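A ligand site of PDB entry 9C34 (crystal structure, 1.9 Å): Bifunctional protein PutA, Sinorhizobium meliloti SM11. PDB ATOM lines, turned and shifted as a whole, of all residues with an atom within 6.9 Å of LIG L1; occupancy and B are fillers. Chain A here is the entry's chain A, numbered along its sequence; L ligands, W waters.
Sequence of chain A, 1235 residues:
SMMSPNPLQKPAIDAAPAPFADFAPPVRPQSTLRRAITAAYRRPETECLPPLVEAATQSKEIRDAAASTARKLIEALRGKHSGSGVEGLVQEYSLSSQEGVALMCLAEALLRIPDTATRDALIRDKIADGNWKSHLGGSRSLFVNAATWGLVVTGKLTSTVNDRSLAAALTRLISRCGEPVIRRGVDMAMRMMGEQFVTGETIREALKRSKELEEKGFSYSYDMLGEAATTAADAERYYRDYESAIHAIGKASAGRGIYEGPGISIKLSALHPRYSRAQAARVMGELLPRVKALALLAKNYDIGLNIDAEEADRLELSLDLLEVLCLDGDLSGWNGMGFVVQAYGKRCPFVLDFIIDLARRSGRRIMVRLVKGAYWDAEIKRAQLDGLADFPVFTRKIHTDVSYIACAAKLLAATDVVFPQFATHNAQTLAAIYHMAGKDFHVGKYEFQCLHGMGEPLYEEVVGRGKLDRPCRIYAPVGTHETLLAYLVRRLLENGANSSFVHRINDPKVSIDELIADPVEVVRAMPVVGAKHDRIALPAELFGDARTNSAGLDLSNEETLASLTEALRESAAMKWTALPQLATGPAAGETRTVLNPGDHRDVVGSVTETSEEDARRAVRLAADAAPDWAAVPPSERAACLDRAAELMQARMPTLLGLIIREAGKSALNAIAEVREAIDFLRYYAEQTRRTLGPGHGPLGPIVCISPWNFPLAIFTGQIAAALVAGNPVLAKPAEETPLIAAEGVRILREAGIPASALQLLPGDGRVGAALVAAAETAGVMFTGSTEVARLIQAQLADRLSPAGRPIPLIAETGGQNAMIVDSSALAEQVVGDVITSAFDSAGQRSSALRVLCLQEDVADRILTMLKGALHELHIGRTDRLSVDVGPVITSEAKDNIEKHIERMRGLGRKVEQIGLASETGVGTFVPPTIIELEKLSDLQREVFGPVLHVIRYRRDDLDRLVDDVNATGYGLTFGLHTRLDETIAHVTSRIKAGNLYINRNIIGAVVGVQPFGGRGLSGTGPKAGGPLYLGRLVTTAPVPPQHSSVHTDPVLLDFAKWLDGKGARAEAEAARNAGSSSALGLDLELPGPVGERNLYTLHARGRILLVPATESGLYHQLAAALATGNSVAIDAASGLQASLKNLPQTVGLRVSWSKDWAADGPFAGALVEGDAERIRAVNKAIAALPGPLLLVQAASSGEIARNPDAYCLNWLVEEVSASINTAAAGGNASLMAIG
The guanidinium group of Arg 490 lies within salt-bridge range of the side-chain carboxylate of Glu 227, at 2.8 Å.
The side-chain amino group of Lys 267 lies within salt-bridge range of the side-chain carboxylate of Asp 308.
The side-chain hydroxyl of Tyr 475 lies within hydrogen-bond range of the side-chain carboxylate of Asp 308 (2.9 Å).
The side-chain carboxylate (OD2) of Asp 223 is in hydrogen-bond range of the side-chain hydroxyl (OH) of Tyr 475, 2.7 Å away.
NH1 of Arg 369 lies within salt-bridge range of OD1 of Asp 308.
OD1 of Asp 308 lies close to OD1 of Asn 306 (3.0 Å).
A nitrogen (N1) of LIG L1 lies close to a nitrogen (N8) of LG2 L2, at 3.2 Å.
An oxygen (O2) of LIG L1 is in salt-bridge range of the guanidinium group (NE) of Arg 490, 2.8 Å away.
An oxygen (O1) of LIG L1 is in salt-bridge range of the side-chain amino group (NZ) of Lys 267 (3.0 Å).
An oxygen (O2) of LIG L1 lies within salt-bridge range of the guanidinium group (NH2) of Arg 491, 3.0 Å away.
An oxygen (O7) of LG2 L2 is in hydrogen-bond range of the backbone NH (N) of Ala 374 (2.9 Å).
The backbone NH of Ala 309 lies within hydrogen-bond range of an oxygen (O8) of LG2 L2 (3.1 Å).
O of Ala 309 lies within hydrogen-bond range of N7 of LG2 L2, at 2.8 Å.
N1 of LG3 L3 sits close to NH1 of Arg 491, at 3.3 Å.
Residues that only touch LIG L1: Asp 308 (3.6 Å), Ala 374 (3.9 Å) and Tyr 475 (3.1 Å).
Hydrophobic or aromatic side chains within 4 Å of LIG L1: Ala 374 and Tyr 475.
Of the 18 residues printed, 6 come within 4 Å of LIG L1.
The nearest printed residue that does not touch LIG L1 is Leu 451 (4.3 Å).
Water W1 lies within hydrogen-bond range of OH of Tyr 375, O of Ala 309, N1 of LIG L1, NZ of Lys 267 and N7 of LG2 L2.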
ATOM      1  N   ASP A 223       9.562   4.947  -5.556  1.00  0.00           N
ATOM      2  CA  ASP A 223       8.531   5.588  -4.740  1.00  0.00           C
ATOM      3  C   ASP A 223       7.197   4.887  -4.921  1.00  0.00           C
ATOM      4  O   ASP A 223       6.588   4.968  -6.005  1.00  0.00           O
ATOM      5  CB  ASP A 223       8.411   7.065  -5.107  1.00  0.00           C
ATOM      6  CG  ASP A 223       7.137   7.701  -4.535  1.00  0.00           C
ATOM      7  OD1 ASP A 223       6.613   7.195  -3.509  1.00  0.00           O
ATOM      8  OD2 ASP A 223       6.669   8.678  -5.153  1.00  0.00           O
ATOM      9  N   LEU A 225       4.293   5.640  -3.918  1.00  0.00           N
ATOM     10  CA  LEU A 225       3.134   6.521  -4.116  1.00  0.00           C
ATOM     11  C   LEU A 225       2.141   6.467  -2.950  1.00  0.00           C
ATOM     12  O   LEU A 225       0.993   6.872  -3.099  1.00  0.00           O
ATOM     13  CB  LEU A 225       2.425   6.203  -5.440  1.00  0.00           C
ATOM     14  CG  LEU A 225       3.115   6.646  -6.750  1.00  0.00           C
ATOM     15  CD1 LEU A 225       2.266   6.346  -7.983  1.00  0.00           C
ATOM     16  CD2 LEU A 225       3.535   8.117  -6.755  1.00  0.00           C
ATOM     17  N   GLU A 227       0.794   8.142   0.496  1.00  0.00           N
ATOM     18  CA  GLU A 227       0.846   9.323   1.352  1.00  0.00           C
ATOM     19  C   GLU A 227      -0.505   9.566   2.004  1.00  0.00           C
ATOM     20  O   GLU A 227      -1.524   9.011   1.592  1.00  0.00           O
ATOM     21  CB  GLU A 227       1.289  10.572   0.582  1.00  0.00           C
ATOM     22  CG  GLU A 227       0.470  10.925  -0.639  1.00  0.00           C
ATOM     23  CD  GLU A 227       1.043  12.123  -1.373  1.00  0.00           C
ATOM     24  OE1 GLU A 227       1.219  13.177  -0.719  1.00  0.00           O
ATOM     25  OE2 GLU A 227       1.354  11.999  -2.577  1.00  0.00           O
ATOM     26  N   SER A 265      12.248   5.339  -1.461  1.00  0.00           N
ATOM     27  CA  SER A 265      11.840   6.574  -0.791  1.00  0.00           C
ATOM     28  C   SER A 265      10.485   6.357  -0.118  1.00  0.00           C
ATOM     29  O   SER A 265       9.602   5.756  -0.711  1.00  0.00           O
ATOM     30  CB  SER A 265      11.729   7.755  -1.768  1.00  0.00           C
ATOM     31  OG  SER A 265      12.994   8.094  -2.303  1.00  0.00           O
ATOM     32  N   LYS A 267       7.292   8.226   2.543  1.00  0.00           N
ATOM     33  CA  LYS A 267       6.688   9.433   3.105  1.00  0.00           C
ATOM     34  C   LYS A 267       6.180   9.080   4.497  1.00  0.00           C
ATOM     35  O   LYS A 267       5.412   8.131   4.654  1.00  0.00           O
ATOM     36  CB  LYS A 267       5.535   9.938   2.240  1.00  0.00           C
ATOM     37  CG  LYS A 267       6.011  10.644   0.941  1.00  0.00           C
ATOM     38  CD  LYS A 267       4.836  11.236   0.159  1.00  0.00           C
ATOM     39  CE  LYS A 267       5.305  12.271  -0.872  1.00  0.00           C
ATOM     40  NZ  LYS A 267       6.310  11.754  -1.853  1.00  0.00           N
ATOM     41  N   ASN A 306      15.244   6.607   1.886  1.00  0.00           N
ATOM     42  CA  ASN A 306      15.127   8.058   1.942  1.00  0.00           C
ATOM     43  C   ASN A 306      13.768   8.461   2.524  1.00  0.00           C
ATOM     44  O   ASN A 306      12.724   7.951   2.094  1.00  0.00           O
ATOM     45  CB  ASN A 306      15.267   8.660   0.534  1.00  0.00           C
ATOM     46  CG  ASN A 306      14.957  10.132   0.501  1.00  0.00           C
ATOM     47  OD1 ASN A 306      13.819  10.560   0.220  1.00  0.00           O
ATOM     48  ND2 ASN A 306      15.934  10.928   0.841  1.00  0.00           N
ATOM     49  N   ASP A 308      11.183  11.280   2.391  1.00  0.00           N
ATOM     50  CA  ASP A 308      10.743  12.424   1.579  1.00  0.00           C
ATOM     51  C   ASP A 308      10.323  13.595   2.467  1.00  0.00           C
ATOM     52  O   ASP A 308       9.912  13.404   3.602  1.00  0.00           O
ATOM     53  CB  ASP A 308       9.544  12.045   0.694  1.00  0.00           C
ATOM     54  CG  ASP A 308       9.924  11.185  -0.530  1.00  0.00           C
ATOM     55  OD1 ASP A 308      11.122  11.133  -0.876  1.00  0.00           O
ATOM     56  OD2 ASP A 308       9.017  10.567  -1.153  1.00  0.00           O
ATOM     57  N   ALA A 309      10.472  14.822   1.956  1.00  0.00           N
ATOM     58  CA  ALA A 309      10.037  16.024   2.656  1.00  0.00           C
ATOM     59  C   ALA A 309       8.642  16.442   2.216  1.00  0.00           C
ATOM     60  O   ALA A 309       8.332  16.451   1.027  1.00  0.00           O
ATOM     61  CB  ALA A 309      10.970  17.209   2.455  1.00  0.00           C
ATOM     62  N   VAL A 340      15.383  14.315   2.814  1.00  0.00           N
ATOM     63  CA  VAL A 340      15.181  15.386   1.837  1.00  0.00           C
ATOM     64  C   VAL A 340      15.119  16.727   2.556  1.00  0.00           C
ATOM     65  O   VAL A 340      14.484  16.850   3.599  1.00  0.00           O
ATOM     66  CB  VAL A 340      13.871  15.159   1.038  1.00  0.00           C
ATOM     67  CG1 VAL A 340      13.627  16.326   0.035  1.00  0.00           C
ATOM     68  CG2 VAL A 340      13.873  13.834   0.327  1.00  0.00           C
ATOM     69  N   ARG A 369      19.182  14.517   0.087  1.00  0.00           N
ATOM     70  CA  ARG A 369      18.608  14.908  -1.193  1.00  0.00           C
ATOM     71  C   ARG A 369      18.173  16.365  -1.117  1.00  0.00           C
ATOM     72  O   ARG A 369      17.218  16.689  -0.410  1.00  0.00           O
ATOM     73  CB  ARG A 369      17.439  14.012  -1.559  1.00  0.00           C
ATOM     74  CG  ARG A 369      16.901  14.318  -2.966  1.00  0.00           C
ATOM     75  CD  ARG A 369      15.528  13.759  -3.153  1.00  0.00           C
ATOM     76  NE  ARG A 369      15.529  12.305  -3.214  1.00  0.00           N
ATOM     77  CZ  ARG A 369      14.482  11.542  -2.907  1.00  0.00           C
ATOM     78  NH1 ARG A 369      13.334  12.079  -2.545  1.00  0.00           N
ATOM     79  NH2 ARG A 369      14.610  10.209  -2.963  1.00  0.00           N
ATOM     80  N   VAL A 371      16.240  19.296  -2.790  1.00  0.00           N
ATOM     81  CA  VAL A 371      15.212  19.552  -3.795  1.00  0.00           C
ATOM     82  C   VAL A 371      14.835  21.018  -3.670  1.00  0.00           C
ATOM     83  O   VAL A 371      15.191  21.676  -2.701  1.00  0.00           O
ATOM     84  CB  VAL A 371      13.966  18.661  -3.622  1.00  0.00           C
ATOM     85  CG1 VAL A 371      14.327  17.222  -3.600  1.00  0.00           C
ATOM     86  CG2 VAL A 371      13.244  18.995  -2.336  1.00  0.00           C
ATOM     87  N   ALA A 374       7.910  20.917  -3.393  1.00  0.00           N
ATOM     88  CA  ALA A 374       6.764  20.514  -4.196  1.00  0.00           C
ATOM     89  C   ALA A 374       5.427  21.086  -3.755  1.00  0.00           C
ATOM     90  O   ALA A 374       4.422  20.818  -4.422  1.00  0.00           O
ATOM     91  CB  ALA A 374       6.667  18.976  -4.189  1.00  0.00           C
ATOM     92  N   TYR A 375       5.368  21.820  -2.641  1.00  0.00           N
ATOM     93  CA  TYR A 375       4.078  22.186  -2.031  1.00  0.00           C
ATOM     94  C   TYR A 375       3.893  23.709  -1.965  1.00  0.00           C
ATOM     95  O   TYR A 375       3.182  24.217  -1.094  1.00  0.00           O
ATOM     96  CB  TYR A 375       3.956  21.599  -0.627  1.00  0.00           C
ATOM     97  CG  TYR A 375       4.177  20.081  -0.565  1.00  0.00           C
ATOM     98  CD1 TYR A 375       5.454  19.554  -0.455  1.00  0.00           C
ATOM     99  CD2 TYR A 375       3.106  19.214  -0.626  1.00  0.00           C
ATOM    100  CE1 TYR A 375       5.659  18.170  -0.402  1.00  0.00           C
ATOM    101  CE2 TYR A 375       3.283  17.834  -0.563  1.00  0.00           C
ATOM    102  CZ  TYR A 375       4.557  17.314  -0.465  1.00  0.00           C
ATOM    103  OH  TYR A 375       4.687  15.933  -0.424  1.00  0.00           O
ATOM    104  N   LEU A 451      13.529  12.869 -11.961  1.00  0.00           N
ATOM    105  CA  LEU A 451      12.276  12.132 -11.905  1.00  0.00           C
ATOM    106  C   LEU A 451      12.135  11.307 -13.175  1.00  0.00           C
ATOM    107  O   LEU A 451      12.459  11.771 -14.266  1.00  0.00           O
ATOM    108  CB  LEU A 451      11.085  13.073 -11.764  1.00  0.00           C
ATOM    109  CG  LEU A 451      10.940  13.846 -10.434  1.00  0.00           C
ATOM    110  CD1 LEU A 451       9.679  14.710 -10.480  1.00  0.00           C
ATOM    111  CD2 LEU A 451      10.867  12.977  -9.178  1.00  0.00           C
ATOM    112  N   TYR A 475      14.258   8.861  -9.655  1.00  0.00           N
ATOM    113  CA  TYR A 475      13.149   8.658  -8.716  1.00  0.00           C
ATOM    114  C   TYR A 475      11.966   8.068  -9.487  1.00  0.00           C
ATOM    115  O   TYR A 475      11.437   8.690 -10.412  1.00  0.00           O
ATOM    116  CB  TYR A 475      12.796   9.993  -8.051  1.00  0.00           C
ATOM    117  CG  TYR A 475      11.758   9.960  -6.961  1.00  0.00           C
ATOM    118  CD1 TYR A 475      10.404  10.114  -7.275  1.00  0.00           C
ATOM    119  CD2 TYR A 475      12.121   9.824  -5.617  1.00  0.00           C
ATOM    120  CE1 TYR A 475       9.431  10.066  -6.288  1.00  0.00           C
ATOM    121  CE2 TYR A 475      11.140   9.813  -4.597  1.00  0.00           C
ATOM    122  CZ  TYR A 475       9.795   9.958  -4.952  1.00  0.00           C
ATOM    123  OH  TYR A 475       8.776   9.938  -3.995  1.00  0.00           O
ATOM    124  N   TYR A 487      -2.113  12.004  -7.099  1.00  0.00           N
ATOM    125  CA  TYR A 487      -1.238  13.162  -6.938  1.00  0.00           C
ATOM    126  C   TYR A 487      -0.370  13.382  -8.175  1.00  0.00           C
ATOM    127  O   TYR A 487       0.750  13.903  -8.063  1.00  0.00           O
ATOM    128  CB  TYR A 487      -0.326  13.011  -5.713  1.00  0.00           C
ATOM    129  N   ARG A 490       0.053  17.389  -8.637  1.00  0.00           N
ATOM    130  CA  ARG A 490       1.143  18.052  -7.917  1.00  0.00           C
ATOM    131  C   ARG A 490       2.445  17.865  -8.683  1.00  0.00           C
ATOM    132  O   ARG A 490       3.252  18.798  -8.792  1.00  0.00           O
ATOM    133  CB  ARG A 490       1.280  17.510  -6.487  1.00  0.00           C
ATOM    134  CG  ARG A 490       2.433  18.138  -5.685  1.00  0.00           C
ATOM    135  CD  ARG A 490       2.581  17.559  -4.271  1.00  0.00           C
ATOM    136  NE  ARG A 490       3.069  16.188  -4.292  1.00  0.00           N
ATOM    137  CZ  ARG A 490       2.457  15.149  -3.724  1.00  0.00           C
ATOM    138  NH1 ARG A 490       1.350  15.303  -3.002  1.00  0.00           N
ATOM    139  NH2 ARG A 490       2.971  13.932  -3.879  1.00  0.00           N
ATOM    140  N   ARG A 491       2.622  16.696  -9.288  1.00  0.00           N
ATOM    141  CA  ARG A 491       3.852  16.384  -9.992  1.00  0.00           C
ATOM    142  C   ARG A 491       3.925  17.048 -11.354  1.00  0.00           C
ATOM    143  O   ARG A 491       5.023  17.368 -11.814  1.00  0.00           O
ATOM    144  CB  ARG A 491       4.009  14.871 -10.172  1.00  0.00           C
ATOM    145  CG  ARG A 491       5.102  14.479 -11.159  1.00  0.00           C
ATOM    146  CD  ARG A 491       6.536  14.915 -10.766  1.00  0.00           C
ATOM    147  NE  ARG A 491       6.638  15.976  -9.768  1.00  0.00           N
ATOM    148  CZ  ARG A 491       6.595  15.757  -8.460  1.00  0.00           C
ATOM    149  NH1 ARG A 491       6.440  14.544  -7.972  1.00  0.00           N
ATOM    150  NH2 ARG A 491       6.665  16.799  -7.625  1.00  0.00           N
HETATM  151  C1  LIG L   1       6.237  14.466  -4.669  1.00  0.00           C
HETATM  152  N1  LIG L   1       8.297  13.975  -3.323  1.00  0.00           N
HETATM  153  O1  LIG L   1       5.764  13.347  -4.303  1.00  0.00           O
HETATM  154  C2  LIG L   1       7.733  14.787  -4.446  1.00  0.00           C
HETATM  155  C3  LIG L   1       8.627  14.415  -5.656  1.00  0.00           C
HETATM  156  C4  LIG L   1       9.239  13.073  -5.253  1.00  0.00           C
HETATM  157  C5  LIG L   1       9.080  12.999  -3.768  1.00  0.00           C
HETATM  158  O2  LIG L   1       5.622  15.393  -5.219  1.00  0.00           O
HETATM  159  P1  LG2 L   2      12.813  24.534 -11.545  1.00  0.00           P
HETATM  160  O1  LG2 L   2      14.277  25.128 -11.521  1.00  0.00           O
HETATM  161  O2  LG2 L   2      11.850  24.981 -12.587  1.00  0.00           O
HETATM  162  O3  LG2 L   2      12.283  25.007 -10.066  1.00  0.00           O
HETATM  163  C1  LG2 L   2      10.814  25.002  -9.920  1.00  0.00           C
HETATM  164  C2  LG2 L   2      10.640  25.033  -8.418  1.00  0.00           C
HETATM  165  O4  LG2 L   2      10.851  26.396  -7.960  1.00  0.00           O
HETATM  166  C3  LG2 L   2       9.256  24.649  -7.820  1.00  0.00           C
HETATM  167  O5  LG2 L   2       9.193  23.229  -7.752  1.00  0.00           O
HETATM  168  C4  LG2 L   2       9.301  25.337  -6.431  1.00  0.00           C
HETATM  169  O6  LG2 L   2      10.035  24.616  -5.459  1.00  0.00           O
HETATM  170  C5  LG2 L   2      10.074  26.662  -6.760  1.00  0.00           C
HETATM  171  N1  LG2 L   2       9.208  27.794  -7.054  1.00  0.00           N
HETATM  172  C6  LG2 L   2       8.269  28.025  -8.106  1.00  0.00           C
HETATM  173  N2  LG2 L   2       7.678  29.235  -7.985  1.00  0.00           N
HETATM  174  C7  LG2 L   2       8.209  29.836  -6.851  1.00  0.00           C
HETATM  175  C8  LG2 L   2       8.028  31.083  -6.200  1.00  0.00           C
HETATM  176  N3  LG2 L   2       7.145  32.070  -6.643  1.00  0.00           N
HETATM  177  N4  LG2 L   2       8.751  31.347  -5.056  1.00  0.00           N
HETATM  178  C9  LG2 L   2       9.638  30.407  -4.593  1.00  0.00           C
HETATM  179  N5  LG2 L   2       9.903  29.197  -5.144  1.00  0.00           N
HETATM  180  C10 LG2 L   2       9.167  28.948  -6.258  1.00  0.00           C
HETATM  181  N6  LG2 L   2       9.909  17.940  -3.438  1.00  0.00           N
HETATM  182  C11 LG2 L   2       9.547  17.924  -2.068  1.00  0.00           C
HETATM  183  O7  LG2 L   2       8.993  18.912  -1.583  1.00  0.00           O
HETATM  184  N7  LG2 L   2       9.847  16.798  -1.335  1.00  0.00           N
HETATM  185  C12 LG2 L   2      10.524  15.620  -1.864  1.00  0.00           C
HETATM  186  O8  LG2 L   2      10.758  14.668  -1.153  1.00  0.00           O
HETATM  187  C13 LG2 L   2      10.847  15.714  -3.270  1.00  0.00           C
HETATM  188  N8  LG2 L   2      11.446  14.549  -3.864  1.00  0.00           N
HETATM  189  C14 LG2 L   2      12.103  14.810  -5.148  1.00  0.00           C
HETATM  190  C15 LG2 L   2      13.022  13.845  -5.639  1.00  0.00           C
HETATM  191  C16 LG2 L   2      13.631  14.029  -6.897  1.00  0.00           C
HETATM  192  C17 LG2 L   2      14.612  12.987  -7.390  1.00  0.00           C
HETATM  193  C18 LG2 L   2      13.328  15.156  -7.688  1.00  0.00           C
HETATM  194  C19 LG2 L   2      13.967  15.359  -9.052  1.00  0.00           C
HETATM  195  C20 LG2 L   2      12.395  16.118  -7.195  1.00  0.00           C
HETATM  196  C21 LG2 L   2      11.786  15.943  -5.932  1.00  0.00           C
HETATM  197  N9  LG2 L   2      10.848  16.900  -5.391  1.00  0.00           N
HETATM  198  C22 LG2 L   2      10.549  16.844  -4.027  1.00  0.00           C
HETATM  199  C23 LG2 L   2      10.216  17.909  -6.268  1.00  0.00           C
HETATM  200  C24 LG2 L   2      11.114  19.168  -6.306  1.00  0.00           C
HETATM  201  O9  LG2 L   2      10.866  19.833  -5.039  1.00  0.00           O
HETATM  202  C25 LG2 L   2      10.847  20.211  -7.435  1.00  0.00           C
HETATM  203  O10 LG2 L   2       9.477  20.586  -7.248  1.00  0.00           O
HETATM  204  C26 LG2 L   2      11.000  19.715  -8.889  1.00  0.00           C
HETATM  205  O11 LG2 L   2      12.178  18.861  -8.983  1.00  0.00           O
HETATM  206  C27 LG2 L   2      11.167  20.904  -9.893  1.00  0.00           C
HETATM  207  O12 LG2 L   2      12.275  21.714  -9.487  1.00  0.00           O
HETATM  208  P2  LG2 L   2      13.586  21.793 -10.552  1.00  0.00           P
HETATM  209  O13 LG2 L   2      13.675  20.581 -11.421  1.00  0.00           O
HETATM  210  O14 LG2 L   2      14.788  22.402  -9.868  1.00  0.00           O
HETATM  211  O15 LG2 L   2      12.997  22.982 -11.603  1.00  0.00           O
HETATM  212  N1  LG3 L   3       4.818  11.727  -7.393  1.00  0.00           N
HETATM  213  C1  LG3 L   3       3.865  11.872  -8.612  1.00  0.00           C
HETATM  214  C2  LG3 L   3       2.443  11.219  -8.191  1.00  0.00           C
HETATM  215  O1  LG3 L   3       2.188  11.324  -6.970  1.00  0.00           O
HETATM  216  C3  LG3 L   3       4.600  11.178  -9.770  1.00  0.00           C
HETATM  217  C4  LG3 L   3       6.095  11.302  -9.438  1.00  0.00           C
HETATM  218  C5  LG3 L   3       6.199  11.285  -7.928  1.00  0.00           C
HETATM  219  O2  LG3 L   3       1.777  10.738  -9.150  1.00  0.00           O
HETATM  220  O   HOH W   1       7.096  14.837  -0.893  1.00  0.00           O
